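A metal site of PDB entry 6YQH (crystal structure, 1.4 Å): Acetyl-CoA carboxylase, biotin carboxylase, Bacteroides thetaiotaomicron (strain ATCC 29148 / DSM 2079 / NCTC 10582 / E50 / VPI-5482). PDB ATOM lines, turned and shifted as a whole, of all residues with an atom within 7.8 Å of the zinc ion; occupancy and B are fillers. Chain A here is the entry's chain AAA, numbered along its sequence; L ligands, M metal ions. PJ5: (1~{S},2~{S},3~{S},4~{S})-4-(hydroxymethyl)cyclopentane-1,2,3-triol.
OE2 of Glu 337 sits at hydrogen-bond distance from O1' of the ligand (2.9 Å).
SG of Cys 414 is bonded to C6' of the ligand (1.8 Å).
The side-chain amide nitrogen (ND2) of Asn 264 is in hydrogen-bond range of an oxygen (O2') of the ligand (2.9 Å).
The side-chain carboxylate (OE1) of Glu 318 is in hydrogen-bond range of an oxygen (O5') of the ligand (2.8 Å).
A ring nitrogen (NE2) of His 262 lies close to an oxygen (O1') of the ligand (3.4 Å).
OD1 of Asn 340 sits close to OE2 of Glu 337, 3.3 Å away.
SG of Cys 415 lies close to O of Tyr 393, at 3.8 Å.
The backbone NH of Thr 338 sits close to the side-chain sulfur of Cys 415 (3.7 Å).
The side-chain sulfur (SG) of Cys 339 sits close to the side-chain hydroxyl (OG) of Ser 418 (3.2 Å).
OD1 of Asn 264 lies close to O of Cys 339, at 3.4 Å.
The side-chain sulfur (SG) of Cys 414 lies close to the side-chain hydroxyl (OH) of Tyr 393 (3.4 Å).
The backbone carbonyl oxygen of Cys 414 is in hydrogen-bond range of the side-chain hydroxyl of Ser 418, 3.4 Å away.
Of the 21 residues printed, 4 come within 4 Å of the zinc ion.
The zinc ion is bound by OE1 of Glu 337 (2.0 Å), SG of Cys 415 (2.3 Å), SG of Cys 339 (2.4 Å) and SG of Cys 414 (2.5 Å).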
ATOM      1  N   TRP A  79      -2.725   0.931  29.234  1.00  0.00           N
ATOM      2  CA  TRP A  79      -2.781  -0.539  29.373  1.00  0.00           C
ATOM      3  C   TRP A  79      -3.682  -0.888  30.568  1.00  0.00           C
ATOM      4  O   TRP A  79      -4.073  -2.074  30.692  1.00  0.00           O
ATOM      5  CB  TRP A  79      -1.401  -1.105  29.544  1.00  0.00           C
ATOM      6  CG  TRP A  79      -0.430  -0.884  28.414  1.00  0.00           C
ATOM      7  CD1 TRP A  79      -0.542  -0.062  27.325  1.00  0.00           C
ATOM      8  CD2 TRP A  79       0.849  -1.520  28.323  1.00  0.00           C
ATOM      9  NE1 TRP A  79       0.587  -0.120  26.568  1.00  0.00           N
ATOM     10  CE2 TRP A  79       1.461  -1.030  27.150  1.00  0.00           C
ATOM     11  CE3 TRP A  79       1.491  -2.539  29.050  1.00  0.00           C
ATOM     12  CZ2 TRP A  79       2.722  -1.432  26.743  1.00  0.00           C
ATOM     13  CZ3 TRP A  79       2.702  -2.990  28.574  1.00  0.00           C
ATOM     14  CH2 TRP A  79       3.322  -2.428  27.455  1.00  0.00           C
ATOM     15  N   TYR A 164       1.471 -12.815  34.238  1.00  0.00           N
ATOM     16  CA  TYR A 164       2.425 -11.721  34.362  1.00  0.00           C
ATOM     17  C   TYR A 164       1.862 -10.647  35.279  1.00  0.00           C
ATOM     18  O   TYR A 164       2.566 -10.043  36.100  1.00  0.00           O
ATOM     19  CB  TYR A 164       2.740 -11.153  32.963  1.00  0.00           C
ATOM     20  CG  TYR A 164       3.519  -9.880  32.928  1.00  0.00           C
ATOM     21  CD1 TYR A 164       2.912  -8.663  33.090  1.00  0.00           C
ATOM     22  CD2 TYR A 164       4.882  -9.898  32.642  1.00  0.00           C
ATOM     23  CE1 TYR A 164       3.630  -7.478  33.057  1.00  0.00           C
ATOM     24  CE2 TYR A 164       5.609  -8.709  32.540  1.00  0.00           C
ATOM     25  CZ  TYR A 164       4.985  -7.507  32.790  1.00  0.00           C
ATOM     26  OH  TYR A 164       5.710  -6.357  32.735  1.00  0.00           O
ATOM     27  N   HIS A 262      10.676 -13.355  22.708  1.00  0.00           N
ATOM     28  CA  HIS A 262      10.410 -12.112  23.446  1.00  0.00           C
ATOM     29  C   HIS A 262      11.324 -12.085  24.665  1.00  0.00           C
ATOM     30  O   HIS A 262      11.282 -13.020  25.474  1.00  0.00           O
ATOM     31  CB  HIS A 262       8.933 -12.055  23.842  1.00  0.00           C
ATOM     32  CG  HIS A 262       8.594 -10.760  24.504  1.00  0.00           C
ATOM     33  ND1 HIS A 262       8.663 -10.584  25.881  1.00  0.00           N
ATOM     34  CD2 HIS A 262       8.259  -9.550  23.999  1.00  0.00           C
ATOM     35  CE1 HIS A 262       8.347  -9.326  26.165  1.00  0.00           C
ATOM     36  NE2 HIS A 262       8.105  -8.668  25.020  1.00  0.00           N
ATOM     37  N   ASN A 264      12.071  -9.942  27.517  1.00  0.00           N
ATOM     38  CA  ASN A 264      11.678  -9.697  28.910  1.00  0.00           C
ATOM     39  C   ASN A 264      10.761 -10.801  29.432  1.00  0.00           C
ATOM     40  O   ASN A 264      10.600 -10.896  30.634  1.00  0.00           O
ATOM     41  CB  ASN A 264      11.083  -8.320  29.154  1.00  0.00           C
ATOM     42  CG  ASN A 264      11.096  -7.934  30.618  1.00  0.00           C
ATOM     43  OD1 ASN A 264      12.193  -7.877  31.181  1.00  0.00           O
ATOM     44  ND2 ASN A 264       9.919  -7.714  31.185  1.00  0.00           N
ATOM     45  N   GLU A 318      11.639  -5.588  21.317  1.00  0.00           N
ATOM     46  CA  GLU A 318      11.327  -6.458  22.476  1.00  0.00           C
ATOM     47  C   GLU A 318      11.816  -7.894  22.271  1.00  0.00           C
ATOM     48  O   GLU A 318      11.605  -8.680  23.230  1.00  0.00           O
ATOM     49  CB  GLU A 318       9.845  -6.479  22.909  1.00  0.00           C
ATOM     50  CG  GLU A 318       9.264  -5.086  23.043  1.00  0.00           C
ATOM     51  CD  GLU A 318       7.827  -5.083  23.566  1.00  0.00           C
ATOM     52  OE1 GLU A 318       7.292  -6.200  23.871  1.00  0.00           O
ATOM     53  OE2 GLU A 318       7.180  -3.973  23.541  1.00  0.00           O
ATOM     54  N   GLU A 337      14.814  -2.404  25.263  1.00  0.00           N
ATOM     55  CA  GLU A 337      13.718  -2.119  26.162  1.00  0.00           C
ATOM     56  C   GLU A 337      14.230  -2.008  27.598  1.00  0.00           C
ATOM     57  O   GLU A 337      15.060  -2.829  28.016  1.00  0.00           O
ATOM     58  CB  GLU A 337      12.675  -3.213  26.052  1.00  0.00           C
ATOM     59  CG  GLU A 337      11.517  -3.047  26.947  1.00  0.00           C
ATOM     60  CD  GLU A 337      10.496  -4.160  27.045  1.00  0.00           C
ATOM     61  OE1 GLU A 337       9.745  -4.119  28.029  1.00  0.00           O
ATOM     62  OE2 GLU A 337      10.478  -5.098  26.227  1.00  0.00           O
ATOM     63  N   THR A 338      13.705  -1.063  28.372  1.00  0.00           N
ATOM     64  CA  THR A 338      14.283  -0.837  29.702  1.00  0.00           C
ATOM     65  C   THR A 338      14.002  -2.009  30.676  1.00  0.00           C
ATOM     66  O   THR A 338      14.915  -2.376  31.436  1.00  0.00           O
ATOM     67  CB  THR A 338      13.837   0.507  30.257  1.00  0.00           C
ATOM     68  OG1 THR A 338      13.815   1.485  29.224  1.00  0.00           O
ATOM     69  CG2 THR A 338      14.729   0.962  31.383  1.00  0.00           C
ATOM     70  N   CYS A 339      12.803  -2.573  30.659  1.00  0.00           N
ATOM     71  CA  CYS A 339      12.498  -3.724  31.543  1.00  0.00           C
ATOM     72  C   CYS A 339      13.638  -4.736  31.482  1.00  0.00           C
ATOM     73  O   CYS A 339      14.009  -5.282  32.534  1.00  0.00           O
ATOM     74  CB  CYS A 339      11.233  -4.463  31.161  1.00  0.00           C
ATOM     75  SG  CYS A 339       9.678  -3.607  31.554  1.00  0.00           S
ATOM     76  N   ASN A 340      14.132  -5.023  30.284  1.00  0.00           N
ATOM     77  CA  ASN A 340      15.055  -6.147  30.131  1.00  0.00           C
ATOM     78  C   ASN A 340      16.299  -5.858  30.987  1.00  0.00           C
ATOM     79  O   ASN A 340      16.884  -6.810  31.528  1.00  0.00           O
ATOM     80  CB  ASN A 340      15.448  -6.329  28.670  1.00  0.00           C
ATOM     81  CG  ASN A 340      14.326  -6.377  27.681  1.00  0.00           C
ATOM     82  OD1 ASN A 340      13.224  -5.913  27.937  1.00  0.00           O
ATOM     83  ND2 ASN A 340      14.642  -6.874  26.513  1.00  0.00           N
ATOM     84  N   ASN A 343      15.718  -6.264  34.615  1.00  0.00           N
ATOM     85  CA  ASN A 343      15.706  -7.692  34.972  1.00  0.00           C
ATOM     86  C   ASN A 343      17.108  -8.277  34.894  1.00  0.00           C
ATOM     87  O   ASN A 343      17.501  -9.106  35.772  1.00  0.00           O
ATOM     88  CB  ASN A 343      14.668  -8.454  34.155  1.00  0.00           C
ATOM     89  CG  ASN A 343      13.291  -8.336  34.808  1.00  0.00           C
ATOM     90  OD1 ASN A 343      13.168  -8.511  36.061  1.00  0.00           O
ATOM     91  ND2 ASN A 343      12.242  -8.001  34.026  1.00  0.00           N
ATOM     92  N   VAL A 392      11.568   5.924  30.023  1.00  0.00           N
ATOM     93  CA  VAL A 392      11.801   5.451  28.647  1.00  0.00           C
ATOM     94  C   VAL A 392      11.405   3.967  28.546  1.00  0.00           C
ATOM     95  O   VAL A 392      11.740   3.182  29.436  1.00  0.00           O
ATOM     96  CB  VAL A 392      13.257   5.696  28.234  1.00  0.00           C
ATOM     97  CG1 VAL A 392      13.555   5.145  26.825  1.00  0.00           C
ATOM     98  CG2 VAL A 392      13.553   7.164  28.282  1.00  0.00           C
ATOM     99  N   TYR A 393      10.777   3.616  27.419  1.00  0.00           N
ATOM    100  CA  TYR A 393      10.490   2.216  27.035  1.00  0.00           C
ATOM    101  C   TYR A 393      11.623   1.739  26.120  1.00  0.00           C
ATOM    102  O   TYR A 393      12.273   0.753  26.431  1.00  0.00           O
ATOM    103  CB  TYR A 393       9.123   2.167  26.364  1.00  0.00           C
ATOM    104  CG  TYR A 393       8.438   0.815  26.221  1.00  0.00           C
ATOM    105  CD1 TYR A 393       8.996  -0.176  25.461  1.00  0.00           C
ATOM    106  CD2 TYR A 393       7.237   0.552  26.843  1.00  0.00           C
ATOM    107  CE1 TYR A 393       8.348  -1.387  25.291  1.00  0.00           C
ATOM    108  CE2 TYR A 393       6.544  -0.625  26.641  1.00  0.00           C
ATOM    109  CZ  TYR A 393       7.120  -1.597  25.866  1.00  0.00           C
ATOM    110  OH  TYR A 393       6.404  -2.778  25.713  1.00  0.00           O
ATOM    111  N   PHE A 394      11.792   2.383  24.953  1.00  0.00           N
ATOM    112  CA  PHE A 394      12.805   1.988  23.977  1.00  0.00           C
ATOM    113  C   PHE A 394      13.904   3.042  23.926  1.00  0.00           C
ATOM    114  O   PHE A 394      13.575   4.245  23.791  1.00  0.00           O
ATOM    115  CB  PHE A 394      12.197   1.848  22.585  1.00  0.00           C
ATOM    116  CG  PHE A 394      11.260   0.661  22.438  1.00  0.00           C
ATOM    117  CD1 PHE A 394      11.694  -0.666  22.671  1.00  0.00           C
ATOM    118  CD2 PHE A 394       9.999   0.832  21.930  1.00  0.00           C
ATOM    119  CE1 PHE A 394      10.834  -1.717  22.499  1.00  0.00           C
ATOM    120  CE2 PHE A 394       9.116  -0.240  21.738  1.00  0.00           C
ATOM    121  CZ  PHE A 394       9.564  -1.524  21.994  1.00  0.00           C
ATOM    122  N   TRP A 413       2.710   1.474  30.895  1.00  0.00           N
ATOM    123  CA  TRP A 413       3.543   0.456  30.219  1.00  0.00           C
ATOM    124  C   TRP A 413       4.296  -0.445  31.200  1.00  0.00           C
ATOM    125  O   TRP A 413       4.590  -0.048  32.322  1.00  0.00           O
ATOM    126  CB  TRP A 413       4.542   1.145  29.318  1.00  0.00           C
ATOM    127  CG  TRP A 413       4.102   2.346  28.588  1.00  0.00           C
ATOM    128  CD1 TRP A 413       2.885   2.569  27.964  1.00  0.00           C
ATOM    129  CD2 TRP A 413       4.939   3.472  28.279  1.00  0.00           C
ATOM    130  NE1 TRP A 413       2.885   3.828  27.401  1.00  0.00           N
ATOM    131  CE2 TRP A 413       4.119   4.398  27.581  1.00  0.00           C
ATOM    132  CE3 TRP A 413       6.218   3.859  28.624  1.00  0.00           C
ATOM    133  CZ2 TRP A 413       4.589   5.634  27.182  1.00  0.00           C
ATOM    134  CZ3 TRP A 413       6.703   5.065  28.193  1.00  0.00           C
ATOM    135  CH2 TRP A 413       5.890   5.952  27.483  1.00  0.00           C
ATOM    136  N   CYS A 414       4.721  -1.600  30.703  1.00  0.00           N
ATOM    137  CA  CYS A 414       5.663  -2.456  31.459  1.00  0.00           C
ATOM    138  C   CYS A 414       6.860  -1.618  31.923  1.00  0.00           C
ATOM    139  O   CYS A 414       7.308  -1.777  33.077  1.00  0.00           O
ATOM    140  CB  CYS A 414       6.080  -3.710  30.716  1.00  0.00           C
ATOM    141  SG  CYS A 414       6.715  -3.364  29.030  1.00  0.00           S
ATOM    142  N   CYS A 415       7.439  -0.817  31.058  1.00  0.00           N
ATOM    143  CA  CYS A 415       8.602   0.009  31.367  1.00  0.00           C
ATOM    144  C   CYS A 415       8.288   1.153  32.323  1.00  0.00           C
ATOM    145  O   CYS A 415       9.240   1.694  32.915  1.00  0.00           O
ATOM    146  CB  CYS A 415       9.289   0.496  30.087  1.00  0.00           C
ATOM    147  SG  CYS A 415      10.080  -0.785  29.071  1.00  0.00           S
ATOM    148  N   VAL A 416       7.018   1.515  32.542  1.00  0.00           N
ATOM    149  CA  VAL A 416       6.685   2.420  33.651  1.00  0.00           C
ATOM    150  C   VAL A 416       6.787   1.620  34.943  1.00  0.00           C
ATOM    151  O   VAL A 416       7.304   2.135  35.926  1.00  0.00           O
ATOM    152  CB  VAL A 416       5.315   3.058  33.475  1.00  0.00           C
ATOM    153  CG1 VAL A 416       4.831   3.767  34.724  1.00  0.00           C
ATOM    154  CG2 VAL A 416       5.262   3.992  32.303  1.00  0.00           C
ATOM    155  N   GLY A 417       6.221   0.433  34.975  1.00  0.00           N
ATOM    156  CA  GLY A 417       6.244  -0.398  36.213  1.00  0.00           C
ATOM    157  C   GLY A 417       7.668  -0.644  36.664  1.00  0.00           C
ATOM    158  O   GLY A 417       7.997  -0.361  37.818  1.00  0.00           O
ATOM    159  N   SER A 418       8.533  -1.128  35.785  1.00  0.00           N
ATOM    160  CA  SER A 418       9.962  -1.331  36.142  1.00  0.00           C
ATOM    161  C   SER A 418      10.664   0.012  36.396  1.00  0.00           C
ATOM    162  O   SER A 418      11.509   0.094  37.293  1.00  0.00           O
ATOM    163  CB  SER A 418      10.670  -2.170  35.099  1.00  0.00           C
ATOM    164  OG  SER A 418      10.580  -1.569  33.827  1.00  0.00           O
ATOM    165  N   GLY A 419      10.264   1.055  35.670  1.00  0.00           N
ATOM    166  CA  GLY A 419      10.814   2.384  35.855  1.00  0.00           C
ATOM    167  C   GLY A 419      10.598   2.861  37.278  1.00  0.00           C
ATOM    168  O   GLY A 419      11.534   3.437  37.894  1.00  0.00           O
ATOM    169  N   HIS A 580       4.339   4.688  23.514  1.00  0.00           N
ATOM    170  CA  HIS A 580       5.706   4.486  24.058  1.00  0.00           C
ATOM    171  C   HIS A 580       6.782   4.543  22.955  1.00  0.00           C
ATOM    172  O   HIS A 580       7.944   4.490  23.278  1.00  0.00           O
ATOM    173  CB  HIS A 580       5.760   3.117  24.781  1.00  0.00           C
ATOM    174  CG  HIS A 580       5.443   1.934  23.932  1.00  0.00           C
ATOM    175  ND1 HIS A 580       4.168   1.676  23.405  1.00  0.00           N
ATOM    176  CD2 HIS A 580       6.252   0.945  23.488  1.00  0.00           C
ATOM    177  CE1 HIS A 580       4.253   0.601  22.666  1.00  0.00           C
ATOM    178  NE2 HIS A 580       5.509   0.097  22.751  1.00  0.00           N
HETATM  179  O1' PJ5 L   1       8.511  -6.683  27.700  1.00  0.00           O
HETATM  180  C1' PJ5 L   1       7.752  -6.081  28.739  1.00  0.00           C
HETATM  181  C6' PJ5 L   1       6.769  -5.009  28.236  1.00  0.00           C
HETATM  182  C2' PJ5 L   1       6.879  -7.168  29.347  1.00  0.00           C
HETATM  183  O2' PJ5 L   1       7.558  -8.366  29.656  1.00  0.00           O
HETATM  184  C3' PJ5 L   1       5.719  -7.294  28.376  1.00  0.00           C
HETATM  185  O3' PJ5 L   1       4.544  -8.000  28.916  1.00  0.00           O
HETATM  186  C4' PJ5 L   1       5.419  -5.844  28.032  1.00  0.00           C
HETATM  187  C5' PJ5 L   1       4.898  -5.714  26.601  1.00  0.00           C
HETATM  188  O5' PJ5 L   1       5.241  -6.691  25.694  1.00  0.00           O
HETATM  189 ZN    ZN M   1       9.122  -2.812  29.411  1.00  0.00          ZN
